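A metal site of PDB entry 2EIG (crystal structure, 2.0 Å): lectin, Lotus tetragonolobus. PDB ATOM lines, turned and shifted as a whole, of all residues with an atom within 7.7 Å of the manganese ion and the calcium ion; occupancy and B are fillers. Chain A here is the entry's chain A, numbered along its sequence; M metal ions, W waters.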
ATOM      1  N   THR A  79       7.264   8.714  10.883  1.00  0.00           N
ATOM      2  CA  THR A  79       8.346   7.868  10.396  1.00  0.00           C
ATOM      3  C   THR A  79       9.349   8.764   9.697  1.00  0.00           C
ATOM      4  O   THR A  79       9.011   9.876   9.370  1.00  0.00           O
ATOM      5  CB  THR A  79       7.908   6.712   9.441  1.00  0.00           C
ATOM      6  OG1 THR A  79       7.900   7.094   8.072  1.00  0.00           O
ATOM      7  CG2 THR A  79       6.597   6.147   9.830  1.00  0.00           C
ATOM      8  N   ASP A  80      10.594   8.310   9.529  1.00  0.00           N
ATOM      9  CA  ASP A  80      11.031   7.004  10.050  1.00  0.00           C
ATOM     10  C   ASP A  80      12.092   7.151  11.103  1.00  0.00           C
ATOM     11  O   ASP A  80      12.250   6.304  11.948  1.00  0.00           O
ATOM     12  CB  ASP A  80      11.566   6.148   8.890  1.00  0.00           C
ATOM     13  CG  ASP A  80      10.507   5.231   8.320  1.00  0.00           C
ATOM     14  OD1 ASP A  80      10.341   4.164   8.923  1.00  0.00           O
ATOM     15  OD2 ASP A  80       9.863   5.598   7.290  1.00  0.00           O
ATOM     16  N   GLY A  81      12.889   8.192  11.021  1.00  0.00           N
ATOM     17  CA  GLY A  81      13.813   8.464  12.084  1.00  0.00           C
ATOM     18  C   GLY A  81      14.935   9.243  11.519  1.00  0.00           C
ATOM     19  O   GLY A  81      14.955   9.515  10.336  1.00  0.00           O
ATOM     20  N   GLY A  99      12.552   4.720   3.810  1.00  0.00           N
ATOM     21  CA  GLY A  99      11.671   4.378   4.927  1.00  0.00           C
ATOM     22  C   GLY A  99      12.444   3.885   6.153  1.00  0.00           C
ATOM     23  O   GLY A  99      13.369   4.559   6.662  1.00  0.00           O
ATOM     24  N   GLY A 100      12.058   2.703   6.612  1.00  0.00           N
ATOM     25  CA  GLY A 100      12.583   2.159   7.845  1.00  0.00           C
ATOM     26  C   GLY A 100      14.056   1.748   7.795  1.00  0.00           C
ATOM     27  O   GLY A 100      14.643   1.455   8.846  1.00  0.00           O
ATOM     28  N   TYR A 101      14.606   1.706   6.576  1.00  0.00           N
ATOM     29  CA  TYR A 101      16.055   1.443   6.354  1.00  0.00           C
ATOM     30  C   TYR A 101      16.924   2.684   6.574  1.00  0.00           C
ATOM     31  O   TYR A 101      18.143   2.608   6.503  1.00  0.00           O
ATOM     32  CB  TYR A 101      16.305   0.833   4.994  1.00  0.00           C
ATOM     33  CG  TYR A 101      15.641  -0.511   4.877  1.00  0.00           C
ATOM     34  CD1 TYR A 101      16.172  -1.616   5.596  1.00  0.00           C
ATOM     35  CD2 TYR A 101      14.465  -0.676   4.122  1.00  0.00           C
ATOM     36  CE1 TYR A 101      15.544  -2.859   5.560  1.00  0.00           C
ATOM     37  CE2 TYR A 101      13.821  -1.938   4.073  1.00  0.00           C
ATOM     38  CZ  TYR A 101      14.378  -3.022   4.791  1.00  0.00           C
ATOM     39  OH  TYR A 101      13.808  -4.300   4.782  1.00  0.00           O
ATOM     40  N   LEU A 102      16.267   3.818   6.876  1.00  0.00           N
ATOM     41  CA  LEU A 102      16.904   5.011   7.437  1.00  0.00           C
ATOM     42  C   LEU A 102      17.969   5.690   6.575  1.00  0.00           C
ATOM     43  O   LEU A 102      18.681   6.556   7.057  1.00  0.00           O
ATOM     44  CB  LEU A 102      17.392   4.774   8.899  1.00  0.00           C
ATOM     45  CG  LEU A 102      16.223   4.563   9.896  1.00  0.00           C
ATOM     46  CD1 LEU A 102      16.671   4.040  11.249  1.00  0.00           C
ATOM     47  CD2 LEU A 102      15.332   5.837  10.123  1.00  0.00           C
ATOM     48  N   GLU A 118      20.498   5.557  16.060  1.00  0.00           N
ATOM     49  CA  GLU A 118      19.250   5.867  15.406  1.00  0.00           C
ATOM     50  C   GLU A 118      18.241   6.344  16.418  1.00  0.00           C
ATOM     51  O   GLU A 118      18.204   5.926  17.562  1.00  0.00           O
ATOM     52  CB  GLU A 118      18.665   4.657  14.626  1.00  0.00           C
ATOM     53  CG  GLU A 118      18.291   3.520  15.576  1.00  0.00           C
ATOM     54  CD  GLU A 118      17.510   2.410  14.915  1.00  0.00           C
ATOM     55  OE1 GLU A 118      17.881   1.930  13.837  1.00  0.00           O
ATOM     56  OE2 GLU A 118      16.520   2.011  15.523  1.00  0.00           O
ATOM     57  N   PHE A 119      17.383   7.218  15.938  1.00  0.00           N
ATOM     58  CA  PHE A 119      16.323   7.760  16.735  1.00  0.00           C
ATOM     59  C   PHE A 119      15.187   7.371  15.793  1.00  0.00           C
ATOM     60  O   PHE A 119      14.921   8.016  14.798  1.00  0.00           O
ATOM     61  CB  PHE A 119      16.474   9.277  16.879  1.00  0.00           C
ATOM     62  CG  PHE A 119      17.663   9.697  17.713  1.00  0.00           C
ATOM     63  CD1 PHE A 119      18.890   9.946  17.118  1.00  0.00           C
ATOM     64  CD2 PHE A 119      17.553   9.804  19.113  1.00  0.00           C
ATOM     65  CE1 PHE A 119      20.000  10.335  17.866  1.00  0.00           C
ATOM     66  CE2 PHE A 119      18.650  10.190  19.866  1.00  0.00           C
ATOM     67  CZ  PHE A 119      19.887  10.463  19.253  1.00  0.00           C
ATOM     68  N   ASP A 120      14.545   6.278  16.127  1.00  0.00           N
ATOM     69  CA  ASP A 120      13.674   5.603  15.227  1.00  0.00           C
ATOM     70  C   ASP A 120      12.256   5.842  15.760  1.00  0.00           C
ATOM     71  O   ASP A 120      11.947   5.484  16.884  1.00  0.00           O
ATOM     72  CB  ASP A 120      14.038   4.104  15.244  1.00  0.00           C
ATOM     73  CG  ASP A 120      13.266   3.282  14.243  1.00  0.00           C
ATOM     74  OD1 ASP A 120      13.725   2.188  13.876  1.00  0.00           O
ATOM     75  OD2 ASP A 120      12.166   3.655  13.818  1.00  0.00           O
ATOM     76  N   SER A 121      11.423   6.461  14.933  1.00  0.00           N
ATOM     77  CA  SER A 121      10.092   6.917  15.365  1.00  0.00           C
ATOM     78  C   SER A 121       8.994   5.923  14.969  1.00  0.00           C
ATOM     79  O   SER A 121       7.841   6.196  15.140  1.00  0.00           O
ATOM     80  CB  SER A 121       9.796   8.254  14.706  1.00  0.00           C
ATOM     81  OG  SER A 121       9.974   8.179  13.300  1.00  0.00           O
ATOM     82  N   HIS A 122       9.355   4.835  14.305  1.00  0.00           N
ATOM     83  CA  HIS A 122       8.359   3.927  13.723  1.00  0.00           C
ATOM     84  C   HIS A 122       8.767   2.452  13.850  1.00  0.00           C
ATOM     85  O   HIS A 122       9.799   2.066  13.309  1.00  0.00           O
ATOM     86  CB  HIS A 122       8.171   4.243  12.244  1.00  0.00           C
ATOM     87  CG  HIS A 122       7.234   3.302  11.550  1.00  0.00           C
ATOM     88  ND1 HIS A 122       5.869   3.400  11.658  1.00  0.00           N
ATOM     89  CD2 HIS A 122       7.470   2.262  10.709  1.00  0.00           C
ATOM     90  CE1 HIS A 122       5.296   2.451  10.935  1.00  0.00           C
ATOM     91  NE2 HIS A 122       6.246   1.735  10.370  1.00  0.00           N
ATOM     92  N   PRO A 123       7.950   1.635  14.560  1.00  0.00           N
ATOM     93  CA  PRO A 123       8.217   0.196  14.709  1.00  0.00           C
ATOM     94  C   PRO A 123       8.040  -0.554  13.398  1.00  0.00           C
ATOM     95  O   PRO A 123       6.932  -0.692  12.882  1.00  0.00           O
ATOM     96  CB  PRO A 123       7.196  -0.274  15.743  1.00  0.00           C
ATOM     97  CG  PRO A 123       6.659   0.969  16.331  1.00  0.00           C
ATOM     98  CD  PRO A 123       6.725   2.013  15.264  1.00  0.00           C
ATOM     99  N   ASN A 124       9.158  -0.976  12.853  1.00  0.00           N
ATOM    100  CA  ASN A 124       9.170  -1.838  11.704  1.00  0.00           C
ATOM    101  C   ASN A 124       9.192  -3.266  12.278  1.00  0.00           C
ATOM    102  O   ASN A 124       9.320  -3.469  13.487  1.00  0.00           O
ATOM    103  CB  ASN A 124      10.416  -1.557  10.874  1.00  0.00           C
ATOM    104  CG  ASN A 124      10.356  -0.227  10.112  1.00  0.00           C
ATOM    105  OD1 ASN A 124      10.975   0.766  10.536  1.00  0.00           O
ATOM    106  ND2 ASN A 124       9.613  -0.196   9.011  1.00  0.00           N
ATOM    107  N   VAL A 125       9.113  -4.251  11.401  1.00  0.00           N
ATOM    108  CA  VAL A 125       9.112  -5.656  11.788  1.00  0.00           C
ATOM    109  C   VAL A 125      10.360  -6.100  12.576  1.00  0.00           C
ATOM    110  O   VAL A 125      10.268  -7.021  13.390  1.00  0.00           O
ATOM    111  CB  VAL A 125       8.871  -6.582  10.521  1.00  0.00           C
ATOM    112  CG1 VAL A 125       7.603  -6.149   9.773  1.00  0.00           C
ATOM    113  CG2 VAL A 125       9.989  -6.448   9.605  1.00  0.00           C
ATOM    114  N   TRP A 126      11.507  -5.403  12.355  1.00  0.00           N
ATOM    115  CA  TRP A 126      12.797  -5.795  12.898  1.00  0.00           C
ATOM    116  C   TRP A 126      13.141  -4.975  14.122  1.00  0.00           C
ATOM    117  O   TRP A 126      14.180  -5.172  14.769  1.00  0.00           O
ATOM    118  CB  TRP A 126      13.863  -5.578  11.819  1.00  0.00           C
ATOM    119  CG  TRP A 126      13.825  -4.125  11.258  1.00  0.00           C
ATOM    120  CD1 TRP A 126      14.263  -2.997  11.864  1.00  0.00           C
ATOM    121  CD2 TRP A 126      13.267  -3.694   9.986  1.00  0.00           C
ATOM    122  NE1 TRP A 126      14.064  -1.904  11.054  1.00  0.00           N
ATOM    123  CE2 TRP A 126      13.469  -2.305   9.894  1.00  0.00           C
ATOM    124  CE3 TRP A 126      12.637  -4.363   8.927  1.00  0.00           C
ATOM    125  CZ2 TRP A 126      13.066  -1.562   8.785  1.00  0.00           C
ATOM    126  CZ3 TRP A 126      12.228  -3.637   7.833  1.00  0.00           C
ATOM    127  CH2 TRP A 126      12.431  -2.224   7.780  1.00  0.00           C
ATOM    128  N   ASP A 127      12.274  -4.014  14.413  1.00  0.00           N
ATOM    129  CA  ASP A 127      12.412  -3.135  15.540  1.00  0.00           C
ATOM    130  C   ASP A 127      12.020  -3.809  16.830  1.00  0.00           C
ATOM    131  O   ASP A 127      11.293  -4.792  16.805  1.00  0.00           O
ATOM    132  CB  ASP A 127      11.573  -1.873  15.302  1.00  0.00           C
ATOM    133  CG  ASP A 127      12.283  -0.908  14.429  1.00  0.00           C
ATOM    134  OD1 ASP A 127      13.522  -0.921  14.514  1.00  0.00           O
ATOM    135  OD2 ASP A 127      11.628  -0.212  13.626  1.00  0.00           O
ATOM    136  N   PRO A 128      12.521  -3.273  17.951  1.00  0.00           N
ATOM    137  CA  PRO A 128      12.316  -3.935  19.229  1.00  0.00           C
ATOM    138  C   PRO A 128      10.829  -4.261  19.434  1.00  0.00           C
ATOM    139  O   PRO A 128       9.989  -3.353  19.680  1.00  0.00           O
ATOM    140  CB  PRO A 128      12.874  -2.942  20.249  1.00  0.00           C
ATOM    141  CG  PRO A 128      13.858  -2.097  19.510  1.00  0.00           C
ATOM    142  CD  PRO A 128      13.374  -2.070  18.064  1.00  0.00           C
ATOM    143  N   SER A 133       7.648   1.451  20.777  1.00  0.00           N
ATOM    144  CA  SER A 133       7.305   2.170  19.586  1.00  0.00           C
ATOM    145  C   SER A 133       8.637   2.878  19.160  1.00  0.00           C
ATOM    146  O   SER A 133       9.569   2.232  18.634  1.00  0.00           O
ATOM    147  CB  SER A 133       6.179   3.138  19.933  1.00  0.00           C
ATOM    148  OG  SER A 133       5.790   3.905  18.816  1.00  0.00           O
ATOM    149  N   SER A 134       8.742   4.168  19.445  1.00  0.00           N
ATOM    150  CA  SER A 134       9.987   4.897  19.196  1.00  0.00           C
ATOM    151  C   SER A 134      11.069   4.385  20.115  1.00  0.00           C
ATOM    152  O   SER A 134      10.827   4.008  21.261  1.00  0.00           O
ATOM    153  CB  SER A 134       9.800   6.414  19.392  1.00  0.00           C
ATOM    154  OG  SER A 134       8.866   6.892  18.469  1.00  0.00           O
ATOM    155  N   HIS A 135      12.271   4.337  19.588  1.00  0.00           N
ATOM    156  CA  HIS A 135      13.372   3.816  20.331  1.00  0.00           C
ATOM    157  C   HIS A 135      14.673   4.471  19.870  1.00  0.00           C
ATOM    158  O   HIS A 135      14.777   5.002  18.751  1.00  0.00           O
ATOM    159  CB  HIS A 135      13.426   2.308  20.158  1.00  0.00           C
ATOM    160  CG  HIS A 135      13.396   1.856  18.735  1.00  0.00           C
ATOM    161  ND1 HIS A 135      12.251   1.795  17.988  1.00  0.00           N
ATOM    162  CD2 HIS A 135      14.386   1.434  17.936  1.00  0.00           C
ATOM    163  CE1 HIS A 135      12.533   1.345  16.776  1.00  0.00           C
ATOM    164  NE2 HIS A 135      13.839   1.110  16.729  1.00  0.00           N
ATOM    165  N   ILE A 136      15.646   4.470  20.760  1.00  0.00           N
ATOM    166  CA  ILE A 136      16.966   4.952  20.421  1.00  0.00           C
ATOM    167  C   ILE A 136      17.773   3.652  20.302  1.00  0.00           C
ATOM    168  O   ILE A 136      17.747   2.841  21.238  1.00  0.00           O
ATOM    169  CB  ILE A 136      17.509   5.929  21.513  1.00  0.00           C
ATOM    170  CG1 ILE A 136      16.704   7.232  21.535  1.00  0.00           C
ATOM    171  CG2 ILE A 136      19.018   6.273  21.255  1.00  0.00           C
ATOM    172  CD1 ILE A 136      16.423   7.781  23.021  1.00  0.00           C
ATOM    173  N   GLY A 137      18.437   3.446  19.172  1.00  0.00           N
ATOM    174  CA  GLY A 137      19.219   2.233  18.985  1.00  0.00           C
ATOM    175  C   GLY A 137      20.653   2.448  18.568  1.00  0.00           C
ATOM    176  O   GLY A 137      20.964   3.449  17.935  1.00  0.00           O
ATOM    177  N   ASP A 139      23.224   0.706  16.030  1.00  0.00           N
ATOM    178  CA  ASP A 139      23.220  -0.133  14.852  1.00  0.00           C
ATOM    179  C   ASP A 139      24.648  -0.318  14.318  1.00  0.00           C
ATOM    180  O   ASP A 139      25.383   0.672  14.083  1.00  0.00           O
ATOM    181  CB  ASP A 139      22.439   0.524  13.714  1.00  0.00           C
ATOM    182  CG  ASP A 139      21.040   0.894  14.096  1.00  0.00           C
ATOM    183  OD1 ASP A 139      20.475   1.650  13.307  1.00  0.00           O
ATOM    184  OD2 ASP A 139      20.537   0.445  15.160  1.00  0.00           O
ATOM    185  N   ILE A 143      20.119  -2.941  10.290  1.00  0.00           N
ATOM    186  CA  ILE A 143      18.977  -2.106  10.714  1.00  0.00           C
ATOM    187  C   ILE A 143      18.388  -2.619  12.019  1.00  0.00           C
ATOM    188  O   ILE A 143      17.662  -1.912  12.721  1.00  0.00           O
ATOM    189  CB  ILE A 143      17.861  -2.006   9.594  1.00  0.00           C
ATOM    190  CG1 ILE A 143      17.080  -0.687   9.670  1.00  0.00           C
ATOM    191  CG2 ILE A 143      16.898  -3.269   9.624  1.00  0.00           C
ATOM    192  CD1 ILE A 143      17.954   0.645   9.737  1.00  0.00           C
ATOM    193  N   MET A 144      18.700  -3.877  12.364  1.00  0.00           N
ATOM    194  CA  MET A 144      18.300  -4.347  13.684  1.00  0.00           C
ATOM    195  C   MET A 144      19.310  -3.959  14.701  1.00  0.00           C
ATOM    196  O   MET A 144      20.455  -4.434  14.666  1.00  0.00           O
ATOM    197  CB  MET A 144      18.087  -5.866  13.722  1.00  0.00           C
ATOM    198  CG  MET A 144      16.926  -6.275  12.972  1.00  0.00           C
ATOM    199  SD  MET A 144      17.401  -7.655  11.923  1.00  0.00           S
ATOM    200  CE  MET A 144      18.303  -6.758  10.651  1.00  0.00           C
ATOM    201  N   SER A 145      18.885  -3.148  15.649  1.00  0.00           N
ATOM    202  CA  SER A 145      19.791  -2.578  16.614  1.00  0.00           C
ATOM    203  C   SER A 145      20.428  -3.656  17.484  1.00  0.00           C
ATOM    204  O   SER A 145      19.788  -4.653  17.826  1.00  0.00           O
ATOM    205  CB  SER A 145      19.036  -1.580  17.470  1.00  0.00           C
ATOM    206  OG  SER A 145      18.578  -0.564  16.599  1.00  0.00           O
ATOM    207  N   ALA A 148      18.965  -1.333  22.100  1.00  0.00           N
ATOM    208  CA  ALA A 148      18.041  -0.230  21.923  1.00  0.00           C
ATOM    209  C   ALA A 148      17.327   0.057  23.220  1.00  0.00           C
ATOM    210  O   ALA A 148      17.197  -0.805  24.114  1.00  0.00           O
ATOM    211  CB  ALA A 148      17.042  -0.525  20.772  1.00  0.00           C
HETATM  212 MN    MN M   1      14.944   0.633  14.884  1.00  0.00          MN
HETATM  213 CA    CA M   2      11.919   1.743  12.277  1.00  0.00          CA
HETATM  214  O   HOH W   1      13.833   1.100  11.188  1.00  0.00           O
HETATM  215  O   HOH W   2      16.078  -0.933  16.009  1.00  0.00           O
HETATM  216  O   HOH W   3      11.721   3.603  10.865  1.00  0.00           O
HETATM  217  O   HOH W   4      16.047   0.244  13.050  1.00  0.00           O
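The side-chain amide oxygen (OD1) of Asn 124 binds the calcium ion (2.2 Å).
The calcium ion is bound by water W1 (2.3 Å).
Water W3 is bound to the calcium ion, 2.3 Å away.
O of His 122 is bound to the calcium ion (2.4 Å).
OD2 of Asp 127 is bound to the calcium ion (2.4 Å).
OD1 of Asp 120 binds the calcium ion.
The calcium ion is bound by OD2 of Asp 120, at 2.5 Å.
The calcium ion has seven donor atoms within binding distance.
Four residues have an atom within 4 Å of the manganese ion: Glu 118, Asp 120, Asp 127 and His 135.
The manganese ion is bound by the side-chain carboxylate of Asp 127, water W4, the side-chain carboxylate of Glu 118, a ring nitrogen (NE2) of His 135, the side-chain carboxylate of Asp 120 and water W2.
Water W4 lies within hydrogen-bond range of OE1 of Glu 118 and O of Ile 143.
Water W1 bridges O of Gly 100 (2.5 Å) and NE1 of Trp 126 (3.0 Å).
The nearest printed residue that does not touch the calcium ion is Gly 100 (4.4 Å).
The side-chain carboxylate (OE2) of Glu 118 sits close to the side-chain hydroxyl (OG) of Ser 145, at 3.5 Å.
OE1 of Glu 118 lies close to OD1 of Asp 139.
The backbone NH (N) of Glu 118 sits at hydrogen-bond distance from the backbone carbonyl oxygen (O) of Gly 137, at 2.9 Å.
ND1 of His 135 sits at hydrogen-bond distance from O of Ser 133 (2.8 Å).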
